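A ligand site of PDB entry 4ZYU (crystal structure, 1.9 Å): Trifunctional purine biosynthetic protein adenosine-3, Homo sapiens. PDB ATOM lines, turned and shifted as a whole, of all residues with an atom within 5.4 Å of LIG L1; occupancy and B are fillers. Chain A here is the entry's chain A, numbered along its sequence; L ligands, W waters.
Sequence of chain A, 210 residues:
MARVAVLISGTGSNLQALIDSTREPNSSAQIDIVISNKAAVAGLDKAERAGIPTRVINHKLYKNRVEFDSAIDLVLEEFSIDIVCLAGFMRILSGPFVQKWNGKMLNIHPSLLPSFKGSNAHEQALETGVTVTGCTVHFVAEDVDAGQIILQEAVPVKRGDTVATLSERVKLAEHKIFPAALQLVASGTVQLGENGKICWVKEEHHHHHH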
ATOM      1  N   GLY A  10      20.047  29.886 -30.909  1.00  0.00           N
ATOM      2  CA  GLY A  10      20.673  29.419 -32.143  1.00  0.00           C
ATOM      3  C   GLY A  10      20.121  29.972 -33.445  1.00  0.00           C
ATOM      4  O   GLY A  10      19.992  31.186 -33.602  1.00  0.00           O
ATOM      5  N   THR A  11      19.802  29.066 -34.368  1.00  0.00           N
ATOM      6  CA  THR A  11      19.428  29.409 -35.753  1.00  0.00           C
ATOM      7  C   THR A  11      18.318  30.460 -35.852  1.00  0.00           C
ATOM      8  O   THR A  11      18.469  31.467 -36.554  1.00  0.00           O
ATOM      9  CB  THR A  11      18.972  28.144 -36.522  1.00  0.00           C
ATOM     10  OG1 THR A  11      20.078  27.239 -36.660  1.00  0.00           O
ATOM     11  CG2 THR A  11      18.444  28.513 -37.901  1.00  0.00           C
ATOM     12  N   GLY A  12      17.213  30.233 -35.173  1.00  0.00           N
ATOM     13  CA  GLY A  12      16.135  31.200 -35.141  1.00  0.00           C
ATOM     14  C   GLY A  12      15.168  31.115 -36.308  1.00  0.00           C
ATOM     15  O   GLY A  12      14.669  32.136 -36.770  1.00  0.00           O
ATOM     16  N   SER A  13      14.884  29.907 -36.795  1.00  0.00           N
ATOM     17  CA  SER A  13      13.883  29.793 -37.844  1.00  0.00           C
ATOM     18  C   SER A  13      12.497  30.072 -37.264  1.00  0.00           C
ATOM     19  O   SER A  13      11.656  30.688 -37.937  1.00  0.00           O
ATOM     20  CB  SER A  13      13.922  28.417 -38.520  1.00  0.00           C
ATOM     21  OG  SER A  13      13.410  27.411 -37.663  1.00  0.00           O
ATOM     22  N   ASN A  14      12.256  29.651 -36.010  1.00  0.00           N
ATOM     23  CA  ASN A  14      10.986  29.982 -35.352  1.00  0.00           C
ATOM     24  C   ASN A  14      10.869  31.489 -35.088  1.00  0.00           C
ATOM     25  O   ASN A  14       9.807  32.074 -35.257  1.00  0.00           O
ATOM     26  CB  ASN A  14      10.817  29.201 -34.056  1.00  0.00           C
ATOM     27  CG  ASN A  14      10.185  27.832 -34.272  1.00  0.00           C
ATOM     28  OD1 ASN A  14       9.033  27.743 -34.683  1.00  0.00           O
ATOM     29  ND2 ASN A  14      10.930  26.774 -33.995  1.00  0.00           N
ATOM     30  N   LEU A  15      11.972  32.116 -34.698  1.00  0.00           N
ATOM     31  CA  LEU A  15      12.010  33.575 -34.561  1.00  0.00           C
ATOM     32  C   LEU A  15      11.564  34.260 -35.858  1.00  0.00           C
ATOM     33  O   LEU A  15      10.733  35.174 -35.836  1.00  0.00           O
ATOM     34  CB  LEU A  15      13.423  34.056 -34.190  1.00  0.00           C
ATOM     35  CG  LEU A  15      13.601  35.582 -34.218  1.00  0.00           C
ATOM     36  CD1 LEU A  15      12.637  36.279 -33.243  1.00  0.00           C
ATOM     37  CD2 LEU A  15      15.033  35.977 -33.927  1.00  0.00           C
ATOM     38  N   ALA A  87      12.073  30.464 -28.200  1.00  0.00           N
ATOM     39  CA  ALA A  87      12.132  29.983 -29.578  1.00  0.00           C
ATOM     40  C   ALA A  87      13.495  29.363 -29.843  1.00  0.00           C
ATOM     41  O   ALA A  87      14.413  30.037 -30.320  1.00  0.00           O
ATOM     42  CB  ALA A  87      11.843  31.120 -30.559  1.00  0.00           C
ATOM     43  N   GLY A  88      13.617  28.088 -29.509  1.00  0.00           N
ATOM     44  CA  GLY A  88      14.902  27.418 -29.541  1.00  0.00           C
ATOM     45  C   GLY A  88      15.810  27.878 -28.417  1.00  0.00           C
ATOM     46  O   GLY A  88      17.021  27.803 -28.533  1.00  0.00           O
ATOM     47  N   PHE A  89      15.219  28.370 -27.337  1.00  0.00           N
ATOM     48  CA  PHE A  89      15.986  28.731 -26.137  1.00  0.00           C
ATOM     49  C   PHE A  89      16.277  27.462 -25.332  1.00  0.00           C
ATOM     50  O   PHE A  89      15.363  26.813 -24.838  1.00  0.00           O
ATOM     51  CB  PHE A  89      15.198  29.743 -25.291  1.00  0.00           C
ATOM     52  CG  PHE A  89      15.967  30.336 -24.124  1.00  0.00           C
ATOM     53  CD1 PHE A  89      16.885  31.356 -24.328  1.00  0.00           C
ATOM     54  CD2 PHE A  89      15.722  29.908 -22.825  1.00  0.00           C
ATOM     55  CE1 PHE A  89      17.564  31.927 -23.264  1.00  0.00           C
ATOM     56  CE2 PHE A  89      16.414  30.468 -21.748  1.00  0.00           C
ATOM     57  CZ  PHE A  89      17.329  31.490 -21.961  1.00  0.00           C
ATOM     58  N   MET A  90      17.558  27.109 -25.211  1.00  0.00           N
ATOM     59  CA  MET A  90      17.929  25.837 -24.611  1.00  0.00           C
ATOM     60  C   MET A  90      18.499  25.973 -23.190  1.00  0.00           C
ATOM     61  O   MET A  90      19.458  25.275 -22.852  1.00  0.00           O
ATOM     62  CB  MET A  90      18.943  25.091 -25.497  1.00  0.00           C
ATOM     63  CG  MET A  90      18.504  24.882 -26.940  1.00  0.00           C
ATOM     64  SD  MET A  90      16.981  23.914 -27.149  1.00  0.00           S
ATOM     65  CE  MET A  90      17.579  22.265 -26.782  1.00  0.00           C
ATOM     66  N   ASN A 107       6.384  28.297 -25.051  1.00  0.00           N
ATOM     67  CA  ASN A 107       7.522  27.550 -25.562  1.00  0.00           C
ATOM     68  C   ASN A 107       7.077  26.633 -26.694  1.00  0.00           C
ATOM     69  O   ASN A 107       5.971  26.102 -26.647  1.00  0.00           O
ATOM     70  CB  ASN A 107       8.164  26.714 -24.440  1.00  0.00           C
ATOM     71  CG  ASN A 107       9.341  25.882 -24.937  1.00  0.00           C
ATOM     72  OD1 ASN A 107      10.292  26.403 -25.518  1.00  0.00           O
ATOM     73  ND2 ASN A 107       9.276  24.575 -24.701  1.00  0.00           N
ATOM     74  N   ILE A 108       7.925  26.464 -27.709  1.00  0.00           N
ATOM     75  CA  ILE A 108       7.707  25.453 -28.742  1.00  0.00           C
ATOM     76  C   ILE A 108       8.576  24.223 -28.480  1.00  0.00           C
ATOM     77  O   ILE A 108       9.757  24.321 -28.147  1.00  0.00           O
ATOM     78  CB  ILE A 108       7.987  26.015 -30.163  1.00  0.00           C
ATOM     79  CG1 ILE A 108       7.714  24.967 -31.251  1.00  0.00           C
ATOM     80  CG2 ILE A 108       9.424  26.496 -30.278  1.00  0.00           C
ATOM     81  CD1 ILE A 108       6.321  25.007 -31.824  1.00  0.00           C
ATOM     82  N   HIS A 109       7.973  23.045 -28.617  1.00  0.00           N
ATOM     83  CA  HIS A 109       8.683  21.807 -28.334  1.00  0.00           C
ATOM     84  C   HIS A 109       8.423  20.825 -29.464  1.00  0.00           C
ATOM     85  O   HIS A 109       7.278  20.653 -29.868  1.00  0.00           O
ATOM     86  CB  HIS A 109       8.237  21.238 -26.990  1.00  0.00           C
ATOM     87  CG  HIS A 109       8.935  19.977 -26.607  1.00  0.00           C
ATOM     88  ND1 HIS A 109      10.212  19.967 -26.087  1.00  0.00           N
ATOM     89  CD2 HIS A 109       8.561  18.673 -26.711  1.00  0.00           C
ATOM     90  CE1 HIS A 109      10.579  18.714 -25.864  1.00  0.00           C
ATOM     91  NE2 HIS A 109       9.585  17.917 -26.227  1.00  0.00           N
ATOM     92  N   PRO A 110       9.486  20.191 -30.010  1.00  0.00           N
ATOM     93  CA  PRO A 110       9.316  19.365 -31.212  1.00  0.00           C
ATOM     94  C   PRO A 110       8.867  17.928 -30.906  1.00  0.00           C
ATOM     95  O   PRO A 110       9.480  16.970 -31.400  1.00  0.00           O
ATOM     96  CB  PRO A 110      10.714  19.385 -31.854  1.00  0.00           C
ATOM     97  CG  PRO A 110      11.640  19.478 -30.689  1.00  0.00           C
ATOM     98  CD  PRO A 110      10.900  20.306 -29.626  1.00  0.00           C
ATOM     99  N   GLY A 118      12.046  16.929 -22.953  1.00  0.00           N
ATOM    100  CA  GLY A 118      13.492  17.062 -22.871  1.00  0.00           C
ATOM    101  C   GLY A 118      14.130  17.661 -24.107  1.00  0.00           C
ATOM    102  O   GLY A 118      13.438  18.107 -25.020  1.00  0.00           O
ATOM    103  N   SER A 119      15.460  17.647 -24.154  1.00  0.00           N
ATOM    104  CA  SER A 119      16.180  18.413 -25.162  1.00  0.00           C
ATOM    105  C   SER A 119      16.447  17.656 -26.475  1.00  0.00           C
ATOM    106  O   SER A 119      16.909  18.276 -27.449  1.00  0.00           O
ATOM    107  CB  SER A 119      17.513  18.884 -24.591  1.00  0.00           C
ATOM    108  OG  SER A 119      18.351  17.770 -24.370  1.00  0.00           O
ATOM    109  N   HIS A 122      13.585  14.483 -30.956  1.00  0.00           N
ATOM    110  CA  HIS A 122      13.623  13.738 -32.222  1.00  0.00           C
ATOM    111  C   HIS A 122      14.377  12.416 -32.051  1.00  0.00           C
ATOM    112  O   HIS A 122      13.957  11.374 -32.554  1.00  0.00           O
ATOM    113  CB  HIS A 122      14.271  14.573 -33.336  1.00  0.00           C
ATOM    114  CG  HIS A 122      13.457  15.774 -33.721  1.00  0.00           C
ATOM    115  ND1 HIS A 122      12.112  15.697 -34.034  1.00  0.00           N
ATOM    116  CD2 HIS A 122      13.804  17.072 -33.844  1.00  0.00           C
ATOM    117  CE1 HIS A 122      11.676  16.913 -34.329  1.00  0.00           C
ATOM    118  NE2 HIS A 122      12.666  17.760 -34.232  1.00  0.00           N
ATOM    119  N   ASP A 145       8.508  21.224 -19.917  1.00  0.00           N
ATOM    120  CA  ASP A 145       7.599  20.642 -20.930  1.00  0.00           C
ATOM    121  C   ASP A 145       6.331  20.036 -20.327  1.00  0.00           C
ATOM    122  O   ASP A 145       5.798  19.062 -20.863  1.00  0.00           O
ATOM    123  CB  ASP A 145       8.323  19.581 -21.763  1.00  0.00           C
ATOM    124  CG  ASP A 145       9.486  20.145 -22.548  1.00  0.00           C
ATOM    125  OD1 ASP A 145       9.448  21.347 -22.906  1.00  0.00           O
ATOM    126  OD2 ASP A 145      10.439  19.401 -22.808  1.00  0.00           O
ATOM    127  N   LYS A 171       9.888  21.210 -38.270  1.00  0.00           N
ATOM    128  CA  LYS A 171      10.027  22.667 -38.244  1.00  0.00           C
ATOM    129  C   LYS A 171       8.980  23.365 -39.120  1.00  0.00           C
ATOM    130  O   LYS A 171       8.558  24.463 -38.813  1.00  0.00           O
ATOM    131  CB  LYS A 171      11.427  23.093 -38.687  1.00  0.00           C
ATOM    132  CG  LYS A 171      12.427  23.149 -37.543  1.00  0.00           C
ATOM    133  CD  LYS A 171      13.657  23.932 -37.929  1.00  0.00           C
ATOM    134  CE  LYS A 171      14.836  23.556 -37.037  1.00  0.00           C
ATOM    135  NZ  LYS A 171      14.432  23.519 -35.620  1.00  0.00           N
ATOM    136  N   GLU A 174       6.136  23.669 -36.786  1.00  0.00           N
ATOM    137  CA  GLU A 174       6.465  24.652 -35.753  1.00  0.00           C
ATOM    138  C   GLU A 174       6.227  26.080 -36.251  1.00  0.00           C
ATOM    139  O   GLU A 174       5.685  26.928 -35.515  1.00  0.00           O
ATOM    140  CB  GLU A 174       7.915  24.504 -35.305  1.00  0.00           C
ATOM    141  CG  GLU A 174       8.268  23.173 -34.635  1.00  0.00           C
ATOM    142  CD  GLU A 174       9.766  23.097 -34.276  1.00  0.00           C
ATOM    143  OE1 GLU A 174      10.365  24.143 -33.996  1.00  0.00           O
ATOM    144  OE2 GLU A 174      10.344  22.003 -34.300  1.00  0.00           O
ATOM    145  N   HIS A 175       6.600  26.338 -37.498  1.00  0.00           N
ATOM    146  CA  HIS A 175       6.488  27.680 -38.076  1.00  0.00           C
ATOM    147  C   HIS A 175       5.034  28.082 -38.311  1.00  0.00           C
ATOM    148  O   HIS A 175       4.742  29.258 -38.545  1.00  0.00           O
ATOM    149  CB  HIS A 175       7.269  27.772 -39.390  1.00  0.00           C
ATOM    150  CG  HIS A 175       8.731  27.569 -39.223  1.00  0.00           C
ATOM    151  ND1 HIS A 175       9.586  27.340 -40.281  1.00  0.00           N
ATOM    152  CD2 HIS A 175       9.506  27.590 -38.117  1.00  0.00           C
ATOM    153  CE1 HIS A 175      10.816  27.195 -39.828  1.00  0.00           C
ATOM    154  NE2 HIS A 175      10.802  27.358 -38.519  1.00  0.00           N
HETATM  155  C1  LIG L   1      13.104  24.025 -32.671  1.00  0.00           C
HETATM  156  O1  LIG L   1      12.878  22.888 -33.512  1.00  0.00           O
HETATM  157  C2  LIG L   1      12.500  23.746 -31.319  1.00  0.00           C
HETATM  158  O2  LIG L   1      11.351  22.913 -31.446  1.00  0.00           O
HETATM  159  C3  LIG L   1      13.640  23.039 -30.600  1.00  0.00           C
HETATM  160  O3  LIG L   1      14.815  23.718 -31.062  1.00  0.00           O
HETATM  161  C4  LIG L   1      14.594  24.157 -32.416  1.00  0.00           C
HETATM  162  C5  LIG L   1      15.068  25.593 -32.620  1.00  0.00           C
HETATM  163  O4  LIG L   1      15.014  25.940 -34.006  1.00  0.00           O
HETATM  164  N1  LIG L   1      13.502  23.093 -29.157  1.00  0.00           N
HETATM  165  C6  LIG L   1      13.835  22.034 -28.409  1.00  0.00           C
HETATM  166  O5  LIG L   1      14.238  20.980 -28.887  1.00  0.00           O
HETATM  167  C7  LIG L   1      13.679  22.198 -26.915  1.00  0.00           C
HETATM  168  N2  LIG L   1      12.463  22.921 -26.593  1.00  0.00           N
HETATM  169  P1  LIG L   1      15.139  27.469 -34.484  1.00  0.00           P
HETATM  170  O6  LIG L   1      15.346  27.366 -35.982  1.00  0.00           O
HETATM  171  O7  LIG L   1      16.334  28.029 -33.725  1.00  0.00           O
HETATM  172  O8  LIG L   1      13.834  28.091 -34.051  1.00  0.00           O
HETATM  173  C1  LG2 L   2      16.479  20.793 -21.044  1.00  0.00           C
HETATM  174  C2  LG2 L   2      17.465  22.432 -22.527  1.00  0.00           C
HETATM  175  C3  LG2 L   2      16.259  22.528 -23.209  1.00  0.00           C
HETATM  176  N1  LG2 L   2      12.170  26.131 -18.064  1.00  0.00           N
HETATM  177  C4  LG2 L   2      11.155  25.702 -17.303  1.00  0.00           C
HETATM  178  N2  LG2 L   2      10.107  25.047 -17.815  1.00  0.00           N
HETATM  179  C5  LG2 L   2      10.007  24.756 -19.123  1.00  0.00           C
HETATM  180  S1  LG2 L   2      13.166  26.265 -20.554  1.00  0.00           S
HETATM  181  C6  LG2 L   2      12.308  25.543 -21.834  1.00  0.00           C
HETATM  182  C7  LG2 L   2      11.136  24.992 -21.358  1.00  0.00           C
HETATM  183  C8  LG2 L   2      11.008  25.164 -19.986  1.00  0.00           C
HETATM  184  C9  LG2 L   2      12.044  25.837 -19.362  1.00  0.00           C
HETATM  185  O1  LG2 L   2       9.014  24.141 -19.523  1.00  0.00           O
HETATM  186  N3  LG2 L   2      11.180  25.957 -15.905  1.00  0.00           N
HETATM  187  C10 LG2 L   2      17.571  21.560 -21.455  1.00  0.00           C
HETATM  188  C11 LG2 L   2      18.907  21.463 -20.694  1.00  0.00           C
HETATM  189  O2  LG2 L   2      19.879  20.949 -21.199  1.00  0.00           O
HETATM  190  N4  LG2 L   2      18.948  22.001 -19.376  1.00  0.00           N
HETATM  191  C12 LG2 L   2      20.132  21.981 -18.605  1.00  0.00           C
HETATM  192  C13 LG2 L   2      20.331  23.361 -18.007  1.00  0.00           C
HETATM  193  C14 LG2 L   2      20.399  24.357 -19.139  1.00  0.00           C
HETATM  194  C15 LG2 L   2      21.477  23.905 -20.112  1.00  0.00           C
HETATM  195  O3  LG2 L   2      21.178  23.556 -21.285  1.00  0.00           O
HETATM  196  O4  LG2 L   2      22.671  23.864 -19.735  1.00  0.00           O
HETATM  197  C16 LG2 L   2      20.103  20.908 -17.536  1.00  0.00           C
HETATM  198  O5  LG2 L   2      19.148  20.866 -16.707  1.00  0.00           O
HETATM  199  O6  LG2 L   2      21.024  20.055 -17.465  1.00  0.00           O
HETATM  200  C17 LG2 L   2      12.779  25.549 -23.266  1.00  0.00           C
HETATM  201  C18 LG2 L   2      13.711  24.378 -23.487  1.00  0.00           C
HETATM  202  C19 LG2 L   2      12.995  23.076 -23.173  1.00  0.00           C
HETATM  203  C20 LG2 L   2      13.857  21.890 -23.538  1.00  0.00           C
HETATM  204  C21 LG2 L   2      15.170  21.758 -22.811  1.00  0.00           C
HETATM  205  C22 LG2 L   2      15.273  20.903 -21.722  1.00  0.00           C
HETATM  206  O   HOH W   1      14.472  20.758 -33.809  1.00  0.00           O
HETATM  207  O   HOH W   2      11.998  20.224 -35.285  1.00  0.00           O
HETATM  208  O   HOH W   3      13.769  18.509 -27.809  1.00  0.00           O
HETATM  209  O   HOH W   4      12.183  25.715 -28.595  1.00  0.00           O
HETATM  210  O   HOH W   5      13.984  30.477 -33.120  1.00  0.00           O
HETATM  211  O   HOH W   6      17.047  29.905 -31.529  1.00  0.00           O
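Water W5 lies within hydrogen-bond range of O8 of LIG L1 (2.6 Å), O of Ala 87 (2.9 Å), N of Leu 15 (3.0 Å) and N of Asn 14 (3.5 Å).
Water W1 bridges O1 of LIG L1 (2.7 Å) and NZ of Lys 171 (3.3 Å).
Water W6 lies within hydrogen-bond range of O of Ala 87, O7 of LIG L1 and N of Gly 10.
Water W4 lies within hydrogen-bond range of the backbone carbonyl oxygen (O) of Ile 108, the backbone NH (N) of Gly 88 and a nitrogen (N1) of LIG L1.
Water W2 lies within hydrogen-bond range of OE2 of Glu 174, NE2 of His 122 and O1 of LIG L1.
N of Thr 11 touches O7 of LIG L1, 3.7 Å away.
CA of Gly 88 touches C5 of LIG L1 (3.6 Å).
Met 90 touches LIG L1 (SD to C7, 3.7 Å).
His 109 touches LIG L1 (ND1 to N2, 3.7 Å).
Pro 110 touches LIG L1 (CD to O2, 3.2 Å).
Hydrophobic or aromatic side chains that line LIG L1: Met 90 and Pro 110.
11 residues have an atom within 4 Å of LIG L1: Thr 11, Gly 12, Ser 13, Asn 14, Gly 88, Met 90, Ile 108, His 109, Pro 110, Lys 171 and Glu 174.
The nearest printed residue that does not touch LIG L1 is Asn 107 (4.1 Å).
OE1 of Glu 174 is in hydrogen-bond range of ND2 of Asn 14 (2.7 Å).
A ring nitrogen (ND1) of His 109 lies close to the side-chain carboxylate (OD2) of Asp 145, 3.3 Å away.
A ring nitrogen (ND1) of His 175 lies close to the backbone carbonyl oxygen (O) of Lys 171.
A ring nitrogen (NE2) of His 175 is in hydrogen-bond range of the side-chain hydroxyl of Ser 13 (2.7 Å).
The side-chain carboxylate (OE2) of Glu 174 is in hydrogen-bond range of an oxygen (O1) of LIG L1 (2.8 Å).
N of Gly 12 is in hydrogen-bond range of O7 of LIG L1 (2.8 Å).
OG of Ser 13 is in hydrogen-bond range of O6 of LIG L1 (2.6 Å).
The backbone NH (N) of Asn 14 sits at hydrogen-bond distance from an oxygen (O8) of LIG L1 (3.0 Å).
NZ of Lys 171 is in salt-bridge range of O6 of LIG L1, at 3.97 Å.
An oxygen (O3) of LG2 L2 sits close to the backbone carbonyl oxygen (O) of Met 90.
An oxygen (O6) of LIG L1 is in hydrogen-bond range of the backbone NH of Ser 13 (2.7 Å).
An oxygen (O1) of LG2 L2 is in hydrogen-bond range of the backbone NH (N) of Asp 145, at 3.0 Å.
ND2 of Asn 14 sits at hydrogen-bond distance from O8 of LIG L1 (3.2 Å).
O of Ile 108 is in hydrogen-bond range of N2 of LIG L1 (3.4 Å).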
